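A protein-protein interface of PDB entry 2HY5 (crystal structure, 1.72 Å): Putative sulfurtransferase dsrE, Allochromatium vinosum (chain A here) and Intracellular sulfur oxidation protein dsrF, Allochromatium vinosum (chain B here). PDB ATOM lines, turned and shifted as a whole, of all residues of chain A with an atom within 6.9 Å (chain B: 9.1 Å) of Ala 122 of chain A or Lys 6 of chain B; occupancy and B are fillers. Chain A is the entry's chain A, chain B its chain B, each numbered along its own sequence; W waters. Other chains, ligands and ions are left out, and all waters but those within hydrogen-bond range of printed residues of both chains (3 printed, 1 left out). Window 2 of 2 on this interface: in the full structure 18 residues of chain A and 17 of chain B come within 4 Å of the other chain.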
ATOM      1  N   MET A   1     -16.904  14.209 -17.140  1.00  0.00           N
ATOM      2  CA  MET A   1     -16.860  15.491 -16.384  1.00  0.00           C
ATOM      3  C   MET A   1     -15.424  15.964 -16.192  1.00  0.00           C
ATOM      4  O   MET A   1     -14.476  15.234 -16.487  1.00  0.00           O
ATOM      5  CB  MET A   1     -17.526  15.326 -15.015  1.00  0.00           C
ATOM      6  CG  MET A   1     -19.003  14.979 -15.074  1.00  0.00           C
ATOM      7  SD  MET A   1     -19.797  15.124 -13.462  1.00  0.00           S
ATOM      8  CE  MET A   1     -20.649  16.698 -13.649  1.00  0.00           C
ATOM      9  N   LYS A   2     -15.278  17.193 -15.703  1.00  0.00           N
ATOM     10  CA  LYS A   2     -13.970  17.793 -15.451  1.00  0.00           C
ATOM     11  C   LYS A   2     -13.718  17.857 -13.944  1.00  0.00           C
ATOM     12  O   LYS A   2     -14.575  18.303 -13.184  1.00  0.00           O
ATOM     13  CB  LYS A   2     -13.914  19.210 -16.027  1.00  0.00           C
ATOM     14  CG  LYS A   2     -14.241  19.314 -17.505  1.00  0.00           C
ATOM     15  CD  LYS A   2     -14.171  20.765 -17.960  1.00  0.00           C
ATOM     16  CE  LYS A   2     -14.492  20.916 -19.437  1.00  0.00           C
ATOM     17  NZ  LYS A   2     -14.444  22.342 -19.865  1.00  0.00           N
ATOM     18  N   PHE A   3     -12.533  17.420 -13.530  1.00  0.00           N
ATOM     19  CA  PHE A   3     -12.145  17.405 -12.119  1.00  0.00           C
ATOM     20  C   PHE A   3     -11.021  18.361 -11.769  1.00  0.00           C
ATOM     21  O   PHE A   3     -10.124  18.610 -12.570  1.00  0.00           O
ATOM     22  CB  PHE A   3     -11.654  16.015 -11.712  1.00  0.00           C
ATOM     23  CG  PHE A   3     -12.736  14.996 -11.570  1.00  0.00           C
ATOM     24  CD1 PHE A   3     -13.499  14.934 -10.408  1.00  0.00           C
ATOM     25  CD2 PHE A   3     -12.989  14.090 -12.594  1.00  0.00           C
ATOM     26  CE1 PHE A   3     -14.506  13.977 -10.268  1.00  0.00           C
ATOM     27  CE2 PHE A   3     -13.991  13.132 -12.464  1.00  0.00           C
ATOM     28  CZ  PHE A   3     -14.750  13.076 -11.301  1.00  0.00           C
ATOM     29  N   ALA A   4     -11.083  18.879 -10.547  1.00  0.00           N
ATOM     30  CA  ALA A   4     -10.039  19.735 -10.008  1.00  0.00           C
ATOM     31  C   ALA A   4      -9.629  18.935  -8.776  1.00  0.00           C
ATOM     32  O   ALA A   4     -10.466  18.655  -7.918  1.00  0.00           O
ATOM     33  CB  ALA A   4     -10.603  21.090  -9.602  1.00  0.00           C
ATOM     34  N   LEU A   5      -8.365  18.530  -8.698  1.00  0.00           N
ATOM     35  CA  LEU A   5      -7.902  17.758  -7.546  1.00  0.00           C
ATOM     36  C   LEU A   5      -6.951  18.583  -6.695  1.00  0.00           C
ATOM     37  O   LEU A   5      -6.050  19.233  -7.213  1.00  0.00           O
ATOM     38  CB  LEU A   5      -7.190  16.480  -8.000  1.00  0.00           C
ATOM     39  CG  LEU A   5      -7.970  15.531  -8.914  1.00  0.00           C
ATOM     40  CD1 LEU A   5      -7.142  14.277  -9.151  1.00  0.00           C
ATOM     41  CD2 LEU A   5      -9.310  15.170  -8.292  1.00  0.00           C
ATOM     42  N   GLU A  33     -11.939  14.323 -17.573  1.00  0.00           N
ATOM     43  CA  GLU A  33     -10.842  15.263 -17.677  1.00  0.00           C
ATOM     44  C   GLU A  33     -10.406  15.750 -16.300  1.00  0.00           C
ATOM     45  O   GLU A  33     -11.237  16.021 -15.438  1.00  0.00           O
ATOM     46  CB  GLU A  33     -11.273  16.463 -18.515  1.00  0.00           C
ATOM     47  CG  GLU A  33     -10.201  17.524 -18.690  1.00  0.00           C
ATOM     48  CD  GLU A  33     -10.722  18.751 -19.418  1.00  0.00           C
ATOM     49  OE1 GLU A  33     -11.287  18.592 -20.521  1.00  0.00           O
ATOM     50  OE2 GLU A  33     -10.567  19.873 -18.884  1.00  0.00           O
ATOM     51  N   PHE A  35      -8.768  18.763 -14.995  1.00  0.00           N
ATOM     52  CA  PHE A  35      -8.408  20.115 -15.387  1.00  0.00           C
ATOM     53  C   PHE A  35      -7.104  20.587 -14.757  1.00  0.00           C
ATOM     54  O   PHE A  35      -6.334  21.316 -15.383  1.00  0.00           O
ATOM     55  CB  PHE A  35      -9.541  21.072 -15.014  1.00  0.00           C
ATOM     56  CG  PHE A  35      -9.311  22.485 -15.455  1.00  0.00           C
ATOM     57  CD1 PHE A  35      -9.539  22.860 -16.775  1.00  0.00           C
ATOM     58  CD2 PHE A  35      -8.862  23.440 -14.553  1.00  0.00           C
ATOM     59  CE1 PHE A  35      -9.323  24.170 -17.191  1.00  0.00           C
ATOM     60  CE2 PHE A  35      -8.641  24.753 -14.956  1.00  0.00           C
ATOM     61  CZ  PHE A  35      -8.873  25.120 -16.277  1.00  0.00           C
ATOM     62  N   ARG A  36      -6.859  20.171 -13.518  1.00  0.00           N
ATOM     63  CA  ARG A  36      -5.646  20.574 -12.821  1.00  0.00           C
ATOM     64  C   ARG A  36      -5.487  19.803 -11.516  1.00  0.00           C
ATOM     65  O   ARG A  36      -6.472  19.465 -10.864  1.00  0.00           O
ATOM     66  CB  ARG A  36      -5.705  22.080 -12.529  1.00  0.00           C
ATOM     67  CG  ARG A  36      -4.513  22.671 -11.765  1.00  0.00           C
ATOM     68  CD  ARG A  36      -4.575  24.200 -11.824  1.00  0.00           C
ATOM     69  NE  ARG A  36      -4.462  24.647 -13.209  1.00  0.00           N
ATOM     70  CZ  ARG A  36      -5.136  25.659 -13.746  1.00  0.00           C
ATOM     71  NH1 ARG A  36      -5.992  26.366 -13.023  1.00  0.00           N
ATOM     72  NH2 ARG A  36      -4.969  25.944 -15.031  1.00  0.00           N
ATOM     73  N   GLU A 117      -9.334  29.023  -9.669  1.00  0.00           N
ATOM     74  CA  GLU A 117      -9.657  29.015 -11.085  1.00  0.00           C
ATOM     75  C   GLU A 117     -10.138  27.627 -11.514  1.00  0.00           C
ATOM     76  O   GLU A 117     -11.123  27.503 -12.247  1.00  0.00           O
ATOM     77  CB  GLU A 117      -8.420  29.417 -11.892  1.00  0.00           C
ATOM     78  CG  GLU A 117      -8.724  30.336 -13.054  1.00  0.00           C
ATOM     79  CD  GLU A 117      -9.478  29.641 -14.160  1.00  0.00           C
ATOM     80  OE1 GLU A 117     -10.421  30.249 -14.709  1.00  0.00           O
ATOM     81  OE2 GLU A 117      -9.119  28.492 -14.488  1.00  0.00           O
ATOM     82  N   ALA A 118      -9.450  26.588 -11.047  1.00  0.00           N
ATOM     83  CA  ALA A 118      -9.807  25.213 -11.390  1.00  0.00           C
ATOM     84  C   ALA A 118     -11.150  24.821 -10.786  1.00  0.00           C
ATOM     85  O   ALA A 118     -11.928  24.095 -11.408  1.00  0.00           O
ATOM     86  CB  ALA A 118      -8.716  24.244 -10.917  1.00  0.00           C
ATOM     87  N   ALA A 119     -11.412  25.294  -9.569  1.00  0.00           N
ATOM     88  CA  ALA A 119     -12.671  25.004  -8.890  1.00  0.00           C
ATOM     89  C   ALA A 119     -13.826  25.602  -9.680  1.00  0.00           C
ATOM     90  O   ALA A 119     -14.932  25.057  -9.696  1.00  0.00           O
ATOM     91  CB  ALA A 119     -12.653  25.576  -7.471  1.00  0.00           C
ATOM     92  N   ILE A 120     -13.567  26.723 -10.342  1.00  0.00           N
ATOM     93  CA  ILE A 120     -14.589  27.385 -11.144  1.00  0.00           C
ATOM     94  C   ILE A 120     -14.826  26.646 -12.461  1.00  0.00           C
ATOM     95  O   ILE A 120     -15.969  26.456 -12.879  1.00  0.00           O
ATOM     96  CB  ILE A 120     -14.188  28.844 -11.465  1.00  0.00           C
ATOM     97  CG1 ILE A 120     -14.125  29.662 -10.170  1.00  0.00           C
ATOM     98  CG2 ILE A 120     -15.174  29.454 -12.447  1.00  0.00           C
ATOM     99  CD1 ILE A 120     -13.706  31.107 -10.367  1.00  0.00           C
ATOM    100  N   GLN A 121     -13.743  26.221 -13.103  1.00  0.00           N
ATOM    101  CA  GLN A 121     -13.832  25.533 -14.387  1.00  0.00           C
ATOM    102  C   GLN A 121     -14.262  24.074 -14.311  1.00  0.00           C
ATOM    103  O   GLN A 121     -14.956  23.587 -15.201  1.00  0.00           O
ATOM    104  CB  GLN A 121     -12.490  25.615 -15.119  1.00  0.00           C
ATOM    105  CG  GLN A 121     -12.026  27.032 -15.425  1.00  0.00           C
ATOM    106  CD  GLN A 121     -13.019  27.798 -16.280  1.00  0.00           C
ATOM    107  OE1 GLN A 121     -13.535  27.274 -17.268  1.00  0.00           O
ATOM    108  NE2 GLN A 121     -13.279  29.050 -15.911  1.00  0.00           N
ATOM    109  N   ALA A 122     -13.857  23.378 -13.255  1.00  0.00           N
ATOM    110  CA  ALA A 122     -14.193  21.964 -13.102  1.00  0.00           C
ATOM    111  C   ALA A 122     -15.608  21.720 -12.592  1.00  0.00           C
ATOM    112  O   ALA A 122     -16.229  22.591 -11.983  1.00  0.00           O
ATOM    113  CB  ALA A 122     -13.190  21.288 -12.178  1.00  0.00           C
ATOM    114  N   ASP A 123     -16.112  20.522 -12.854  1.00  0.00           N
ATOM    115  CA  ASP A 123     -17.446  20.143 -12.413  1.00  0.00           C
ATOM    116  C   ASP A 123     -17.398  19.680 -10.961  1.00  0.00           C
ATOM    117  O   ASP A 123     -18.362  19.843 -10.217  1.00  0.00           O
ATOM    118  CB  ASP A 123     -17.988  19.016 -13.292  1.00  0.00           C
ATOM    119  CG  ASP A 123     -18.189  19.450 -14.727  1.00  0.00           C
ATOM    120  OD1 ASP A 123     -18.932  20.431 -14.946  1.00  0.00           O
ATOM    121  OD2 ASP A 123     -17.609  18.815 -15.632  1.00  0.00           O
ATOM    122  N   ARG A 124     -16.264  19.110 -10.563  1.00  0.00           N
ATOM    123  CA  ARG A 124     -16.092  18.615  -9.201  1.00  0.00           C
ATOM    124  C   ARG A 124     -14.715  18.956  -8.641  1.00  0.00           C
ATOM    125  O   ARG A 124     -13.714  18.913  -9.358  1.00  0.00           O
ATOM    126  CB  ARG A 124     -16.260  17.095  -9.166  1.00  0.00           C
ATOM    127  CG  ARG A 124     -17.593  16.591  -9.692  1.00  0.00           C
ATOM    128  CD  ARG A 124     -18.725  16.900  -8.736  1.00  0.00           C
ATOM    129  NE  ARG A 124     -19.981  16.319  -9.204  1.00  0.00           N
ATOM    130  CZ  ARG A 124     -20.775  16.877 -10.109  1.00  0.00           C
ATOM    131  NH1 ARG A 124     -20.457  18.042 -10.651  1.00  0.00           N
ATOM    132  NH2 ARG A 124     -21.893  16.263 -10.473  1.00  0.00           N
ATOM    133  N   LEU A 125     -14.683  19.301  -7.358  1.00  0.00           N
ATOM    134  CA  LEU A 125     -13.436  19.604  -6.662  1.00  0.00           C
ATOM    135  C   LEU A 125     -13.275  18.509  -5.619  1.00  0.00           C
ATOM    136  O   LEU A 125     -14.069  18.414  -4.679  1.00  0.00           O
ATOM    137  CB  LEU A 125     -13.505  20.963  -5.963  1.00  0.00           C
ATOM    138  CG  LEU A 125     -12.367  21.261  -4.978  1.00  0.00           C
ATOM    139  CD1 LEU A 125     -11.027  21.363  -5.710  1.00  0.00           C
ATOM    140  CD2 LEU A 125     -12.682  22.548  -4.247  1.00  0.00           C
ATOM    141  N   VAL B   5     -20.721  33.121 -10.051  1.00  0.00           N
ATOM    142  CA  VAL B   5     -21.716  32.178 -10.639  1.00  0.00           C
ATOM    143  C   VAL B   5     -21.889  30.987  -9.704  1.00  0.00           C
ATOM    144  O   VAL B   5     -23.008  30.621  -9.342  1.00  0.00           O
ATOM    145  CB  VAL B   5     -21.257  31.648 -12.014  1.00  0.00           C
ATOM    146  CG1 VAL B   5     -22.452  31.437 -12.926  1.00  0.00           C
ATOM    147  CG2 VAL B   5     -20.256  32.614 -12.637  1.00  0.00           C
ATOM    148  N   LYS B   6     -20.771  30.394  -9.304  1.00  0.00           N
ATOM    149  CA  LYS B   6     -20.796  29.239  -8.417  1.00  0.00           C
ATOM    150  C   LYS B   6     -20.806  29.608  -6.944  1.00  0.00           C
ATOM    151  O   LYS B   6     -20.406  30.702  -6.550  1.00  0.00           O
ATOM    152  CB  LYS B   6     -19.594  28.336  -8.671  1.00  0.00           C
ATOM    153  CG  LYS B   6     -19.698  27.489  -9.918  1.00  0.00           C
ATOM    154  CD  LYS B   6     -18.547  26.506  -9.969  1.00  0.00           C
ATOM    155  CE  LYS B   6     -18.669  25.583 -11.163  1.00  0.00           C
ATOM    156  NZ  LYS B   6     -17.542  24.619 -11.212  1.00  0.00           N
ATOM    157  N   LYS B   7     -21.274  28.665  -6.137  1.00  0.00           N
ATOM    158  CA  LYS B   7     -21.345  28.824  -4.697  1.00  0.00           C
ATOM    159  C   LYS B   7     -20.199  28.035  -4.067  1.00  0.00           C
ATOM    160  O   LYS B   7     -20.177  26.810  -4.133  1.00  0.00           O
ATOM    161  CB  LYS B   7     -22.687  28.296  -4.184  1.00  0.00           C
ATOM    162  CG  LYS B   7     -22.739  28.161  -2.680  1.00  0.00           C
ATOM    163  CD  LYS B   7     -22.316  29.460  -2.040  1.00  0.00           C
ATOM    164  CE  LYS B   7     -22.047  29.295  -0.569  1.00  0.00           C
ATOM    165  NZ  LYS B   7     -21.549  30.573  -0.022  1.00  0.00           N
ATOM    166  N   PHE B   8     -19.254  28.749  -3.460  1.00  0.00           N
ATOM    167  CA  PHE B   8     -18.105  28.122  -2.820  1.00  0.00           C
ATOM    168  C   PHE B   8     -18.176  28.184  -1.301  1.00  0.00           C
ATOM    169  O   PHE B   8     -18.440  29.243  -0.731  1.00  0.00           O
ATOM    170  CB  PHE B   8     -16.804  28.800  -3.260  1.00  0.00           C
ATOM    171  CG  PHE B   8     -16.388  28.479  -4.668  1.00  0.00           C
ATOM    172  CD1 PHE B   8     -15.347  29.180  -5.270  1.00  0.00           C
ATOM    173  CD2 PHE B   8     -17.014  27.466  -5.386  1.00  0.00           C
ATOM    174  CE1 PHE B   8     -14.936  28.879  -6.566  1.00  0.00           C
ATOM    175  CE2 PHE B   8     -16.609  27.157  -6.685  1.00  0.00           C
ATOM    176  CZ  PHE B   8     -15.570  27.864  -7.274  1.00  0.00           C
ATOM    177  N   MET B   9     -17.938  27.048  -0.652  1.00  0.00           N
ATOM    178  CA  MET B   9     -17.931  26.989   0.808  1.00  0.00           C
ATOM    179  C   MET B   9     -16.521  26.679   1.280  1.00  0.00           C
ATOM    180  O   MET B   9     -15.852  25.811   0.726  1.00  0.00           O
ATOM    181  CB  MET B   9     -18.867  25.893   1.342  1.00  0.00           C
ATOM    182  CG  MET B   9     -18.732  25.683   2.858  1.00  0.00           C
ATOM    183  SD  MET B   9     -19.729  24.352   3.570  1.00  0.00           S
ATOM    184  CE  MET B   9     -21.297  25.146   3.655  1.00  0.00           C
ATOM    185  N   TYR B  10     -16.069  27.404   2.296  1.00  0.00           N
ATOM    186  CA  TYR B  10     -14.754  27.183   2.882  1.00  0.00           C
ATOM    187  C   TYR B  10     -15.034  26.571   4.242  1.00  0.00           C
ATOM    188  O   TYR B  10     -15.497  27.259   5.147  1.00  0.00           O
ATOM    189  CB  TYR B  10     -14.016  28.511   3.030  1.00  0.00           C
ATOM    190  CG  TYR B  10     -13.566  29.072   1.706  1.00  0.00           C
ATOM    191  CD1 TYR B  10     -12.345  28.693   1.153  1.00  0.00           C
ATOM    192  CD2 TYR B  10     -14.372  29.955   0.985  1.00  0.00           C
ATOM    193  CE1 TYR B  10     -11.934  29.176  -0.085  1.00  0.00           C
ATOM    194  CE2 TYR B  10     -13.969  30.443  -0.259  1.00  0.00           C
ATOM    195  CZ  TYR B  10     -12.747  30.049  -0.785  1.00  0.00           C
ATOM    196  OH  TYR B  10     -12.334  30.520  -2.012  1.00  0.00           O
ATOM    197  N   PHE B  35     -12.222  36.583  -7.646  1.00  0.00           N
ATOM    198  CA  PHE B  35     -12.963  35.844  -8.657  1.00  0.00           C
ATOM    199  C   PHE B  35     -14.459  36.124  -8.623  1.00  0.00           C
ATOM    200  O   PHE B  35     -15.210  35.604  -9.446  1.00  0.00           O
ATOM    201  CB  PHE B  35     -12.705  34.341  -8.511  1.00  0.00           C
ATOM    202  CG  PHE B  35     -11.288  33.938  -8.804  1.00  0.00           C
ATOM    203  CD1 PHE B  35     -10.276  34.167  -7.876  1.00  0.00           C
ATOM    204  CD2 PHE B  35     -10.959  33.349 -10.024  1.00  0.00           C
ATOM    205  CE1 PHE B  35      -8.955  33.814  -8.153  1.00  0.00           C
ATOM    206  CE2 PHE B  35      -9.642  32.994 -10.312  1.00  0.00           C
ATOM    207  CZ  PHE B  35      -8.637  33.228  -9.373  1.00  0.00           C
ATOM    208  N   ASP B  36     -14.876  36.959  -7.677  1.00  0.00           N
ATOM    209  CA  ASP B  36     -16.278  37.338  -7.507  1.00  0.00           C
ATOM    210  C   ASP B  36     -17.295  36.196  -7.607  1.00  0.00           C
ATOM    211  O   ASP B  36     -18.254  36.270  -8.377  1.00  0.00           O
ATOM    212  CB  ASP B  36     -16.657  38.450  -8.499  1.00  0.00           C
ATOM    213  CG  ASP B  36     -16.387  38.070  -9.945  1.00  0.00           C
ATOM    214  OD1 ASP B  36     -15.204  38.044 -10.348  1.00  0.00           O
ATOM    215  OD2 ASP B  36     -17.357  37.793 -10.682  1.00  0.00           O
ATOM    216  N   GLN B  37     -17.084  35.139  -6.829  1.00  0.00           N
ATOM    217  CA  GLN B  37     -18.016  34.013  -6.815  1.00  0.00           C
ATOM    218  C   GLN B  37     -18.864  34.205  -5.564  1.00  0.00           C
ATOM    219  O   GLN B  37     -18.621  35.134  -4.798  1.00  0.00           O
ATOM    220  CB  GLN B  37     -17.258  32.682  -6.727  1.00  0.00           C
ATOM    221  CG  GLN B  37     -16.324  32.414  -7.899  1.00  0.00           C
ATOM    222  CD  GLN B  37     -17.055  32.390  -9.227  1.00  0.00           C
ATOM    223  OE1 GLN B  37     -17.927  31.552  -9.454  1.00  0.00           O
ATOM    224  NE2 GLN B  37     -16.701  33.313 -10.112  1.00  0.00           N
ATOM    225  N   ASP B  38     -19.864  33.353  -5.367  1.00  0.00           N
ATOM    226  CA  ASP B  38     -20.709  33.444  -4.179  1.00  0.00           C
ATOM    227  C   ASP B  38     -19.945  32.652  -3.129  1.00  0.00           C
ATOM    228  O   ASP B  38     -19.755  31.447  -3.285  1.00  0.00           O
ATOM    229  CB  ASP B  38     -22.067  32.793  -4.436  1.00  0.00           C
ATOM    230  CG  ASP B  38     -23.079  33.109  -3.353  1.00  0.00           C
ATOM    231  OD1 ASP B  38     -22.719  33.045  -2.159  1.00  0.00           O
ATOM    232  OD2 ASP B  38     -24.241  33.412  -3.698  1.00  0.00           O
ATOM    233  N   VAL B  39     -19.517  33.319  -2.063  1.00  0.00           N
ATOM    234  CA  VAL B  39     -18.725  32.657  -1.032  1.00  0.00           C
ATOM    235  C   VAL B  39     -19.283  32.671   0.387  1.00  0.00           C
ATOM    236  O   VAL B  39     -19.915  33.626   0.817  1.00  0.00           O
ATOM    237  CB  VAL B  39     -17.309  33.283  -0.969  1.00  0.00           C
ATOM    238  CG1 VAL B  39     -16.493  32.646   0.148  1.00  0.00           C
ATOM    239  CG2 VAL B  39     -16.613  33.123  -2.310  1.00  0.00           C
ATOM    240  N   CYS B  40     -19.043  31.585   1.109  1.00  0.00           N
ATOM    241  CA  CYS B  40     -19.441  31.515   2.505  1.00  0.00           C
ATOM    242  C   CYS B  40     -18.328  30.777   3.227  1.00  0.00           C
ATOM    243  O   CYS B  40     -17.716  29.855   2.684  1.00  0.00           O
ATOM    244  CB  CYS B  40     -20.786  30.804   2.695  1.00  0.00           C
ATOM    245  SG  CYS B  40     -20.836  29.061   2.287  1.00  0.00           S
ATOM    246  N   GLU B 129     -26.197  23.628  -0.568  1.00  0.00           N
ATOM    247  CA  GLU B 129     -26.290  24.691  -1.563  1.00  0.00           C
ATOM    248  C   GLU B 129     -24.958  24.970  -2.253  1.00  0.00           C
ATOM    249  O   GLU B 129     -24.911  25.678  -3.258  1.00  0.00           O
ATOM    250  CB  GLU B 129     -26.797  25.983  -0.914  1.00  0.00           C
ATOM    251  CG  GLU B 129     -28.191  25.881  -0.315  1.00  0.00           C
ATOM    252  CD  GLU B 129     -28.696  27.212   0.208  1.00  0.00           C
ATOM    253  OE1 GLU B 129     -28.035  27.799   1.092  1.00  0.00           O
ATOM    254  OE2 GLU B 129     -29.758  27.670  -0.265  1.00  0.00           O
ATOM    255  N   SER B 130     -23.881  24.399  -1.731  1.00  0.00           N
ATOM    256  CA  SER B 130     -22.559  24.635  -2.297  1.00  0.00           C
ATOM    257  C   SER B 130     -22.237  23.836  -3.551  1.00  0.00           C
ATOM    258  O   SER B 130     -22.619  22.675  -3.683  1.00  0.00           O
ATOM    259  CB  SER B 130     -21.491  24.363  -1.235  1.00  0.00           C
ATOM    260  OG  SER B 130     -21.716  25.160  -0.083  1.00  0.00           O
ATOM    261  N   ASP B 131     -21.514  24.469  -4.470  1.00  0.00           N
ATOM    262  CA  ASP B 131     -21.117  23.811  -5.708  1.00  0.00           C
ATOM    263  C   ASP B 131     -19.715  23.223  -5.556  1.00  0.00           C
ATOM    264  O   ASP B 131     -19.323  22.307  -6.280  1.00  0.00           O
ATOM    265  CB  ASP B 131     -21.153  24.810  -6.868  1.00  0.00           C
ATOM    266  CG  ASP B 131     -22.549  25.346  -7.126  1.00  0.00           C
ATOM    267  OD1 ASP B 131     -23.482  24.522  -7.249  1.00  0.00           O
ATOM    268  OD2 ASP B 131     -22.717  26.584  -7.212  1.00  0.00           O
ATOM    269  N   ALA B 132     -18.962  23.752  -4.601  1.00  0.00           N
ATOM    270  CA  ALA B 132     -17.613  23.273  -4.345  1.00  0.00           C
ATOM    271  C   ALA B 132     -17.279  23.572  -2.900  1.00  0.00           C
ATOM    272  O   ALA B 132     -17.629  24.633  -2.381  1.00  0.00           O
ATOM    273  CB  ALA B 132     -16.618  23.966  -5.263  1.00  0.00           C
ATOM    274  N   VAL B 133     -16.607  22.633  -2.253  1.00  0.00           N
ATOM    275  CA  VAL B 133     -16.230  22.805  -0.858  1.00  0.00           C
ATOM    276  C   VAL B 133     -14.725  22.662  -0.686  1.00  0.00           C
ATOM    277  O   VAL B 133     -14.143  21.621  -1.007  1.00  0.00           O
ATOM    278  CB  VAL B 133     -16.927  21.763   0.048  1.00  0.00           C
ATOM    279  CG1 VAL B 133     -16.589  22.041   1.514  1.00  0.00           C
ATOM    280  CG2 VAL B 133     -18.437  21.810  -0.166  1.00  0.00           C
ATOM    281  N   PHE B 134     -14.104  23.724  -0.188  1.00  0.00           N
ATOM    282  CA  PHE B 134     -12.676  23.738   0.071  1.00  0.00           C
ATOM    283  C   PHE B 134     -12.487  23.227   1.489  1.00  0.00           C
ATOM    284  O   PHE B 134     -13.044  23.786   2.431  1.00  0.00           O
ATOM    285  CB  PHE B 134     -12.135  25.161  -0.036  1.00  0.00           C
ATOM    286  CG  PHE B 134     -12.085  25.685  -1.440  1.00  0.00           C
ATOM    287  CD1 PHE B 134     -10.996  25.408  -2.255  1.00  0.00           C
ATOM    288  CD2 PHE B 134     -13.134  26.442  -1.952  1.00  0.00           C
ATOM    289  CE1 PHE B 134     -10.944  25.881  -3.562  1.00  0.00           C
ATOM    290  CE2 PHE B 134     -13.093  26.920  -3.261  1.00  0.00           C
ATOM    291  CZ  PHE B 134     -11.996  26.639  -4.068  1.00  0.00           C
HETATM  292  O   HOH W   1     -16.142  20.043  -3.634  1.00  0.00           O
HETATM  293  O   HOH W   2     -19.582  20.065  -7.542  1.00  0.00           O
HETATM  294  O   HOH W   3     -19.428  22.599  -9.696  1.00  0.00           O
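The backbone carbonyl oxygen of Ala 119 of chain A is in hydrogen-bond range of the side-chain amino group of Lys 6 of chain B (3.0 Å).
O of Ile 120 of chain A sits at hydrogen-bond distance from NZ of Lys 6 of chain B.
The backbone carbonyl oxygen (O) of Ala 122 of chain A sits at hydrogen-bond distance from the side-chain amino group (NZ) of Lys 6 of chain B, 2.5 Å away.
The backbone NH (N) of Val 5 of chain B sits at hydrogen-bond distance from the side-chain amide oxygen (OE1) of Gln 37 of chain B, 3.3 Å away.
OE1 of Gln 37 of chain B lies within hydrogen-bond range of N of Lys 6 of chain B (3.1 Å).
O of Lys 6 of chain B sits at hydrogen-bond distance from N of Asp 38 of chain B (3.0 Å).
The backbone carbonyl oxygen (O) of Asp 38 of chain B is in hydrogen-bond range of the backbone NH (N) of Phe 8 of chain B (2.7 Å).
N of Phe 134 of chain B lies within hydrogen-bond range of O of Met 9 of chain B, 2.9 Å away.
O of Phe 35 of chain B sits at hydrogen-bond distance from NE2 of Gln 37 of chain B.
Among the printed residues, pairs that only touch across the chains: Glu 117 of chain A with Phe 35 of chain B (3.9 Å), Ala 119 of chain A with Phe 8 of chain B (3.7 Å), Ala 119 of chain A with Phe 134 of chain B (3.6 Å), Ile 120 of chain A with Phe 8 of chain B (3.7 Å), Ile 120 of chain A with Phe 35 of chain B (3.6 Å), Ile 120 of chain A with Gln 37 of chain B (3.7 Å), Leu 125 of chain A with Val 133 of chain B (3.7 Å) and Leu 125 of chain A with Phe 134 of chain B (3.8 Å).
Printed residues of chain B within 4 Å of Ala 122 of chain A: Lys 6.
Lys 6 of chain B touches just these residues of chain A: Ala 119 (3.0 Å), Ile 120 (2.9 Å) and Ala 122 (2.5 Å).
No residue of chain B comes within 4 Å of Asp 123 of chain A.
Of the printed residues of chain A, Phe 35 of chain B touches Glu 117 (3.9 Å) and Ile 120 (3.6 Å).
Printed residues of chain A within 4 Å of Phe 8 of chain B: Ala 119 and Ile 120.
Phe 3 of chain A touches none of the printed residues of chain B.
Of the 17 printed residues of chain A, 5 touch a printed residue of chain B.
Printed residues of chain A that touch a printed residue of chain B: Glu 117, Ala 119, Ile 120, Ala 122 and Leu 125.
Among the printed residues, 11 pairs touch across the chains.
Among the printed residues, no Asp or Glu carboxylate lies within 4 Å of a Lys or Arg side-chain nitrogen of the other chain.
Water W2 lies within hydrogen-bond range of the backbone carbonyl oxygen (O) of Asp 131 of chain B (2.6 Å) and the backbone carbonyl oxygen (O) of Asp 123 of chain A (2.9 Å).
Water W1 lies within hydrogen-bond range of the backbone carbonyl oxygen (O) of Leu 125 of chain A (2.8 Å) and the backbone NH (N) of Val 133 of chain B (3.0 Å).
Water W3 lies within hydrogen-bond range of the backbone carbonyl oxygen of Asp 123 of chain A (3.0 Å), the side-chain amino group of Lys 6 of chain B (3.2 Å) and the backbone carbonyl oxygen of Asp 131 of chain B (3.4 Å).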
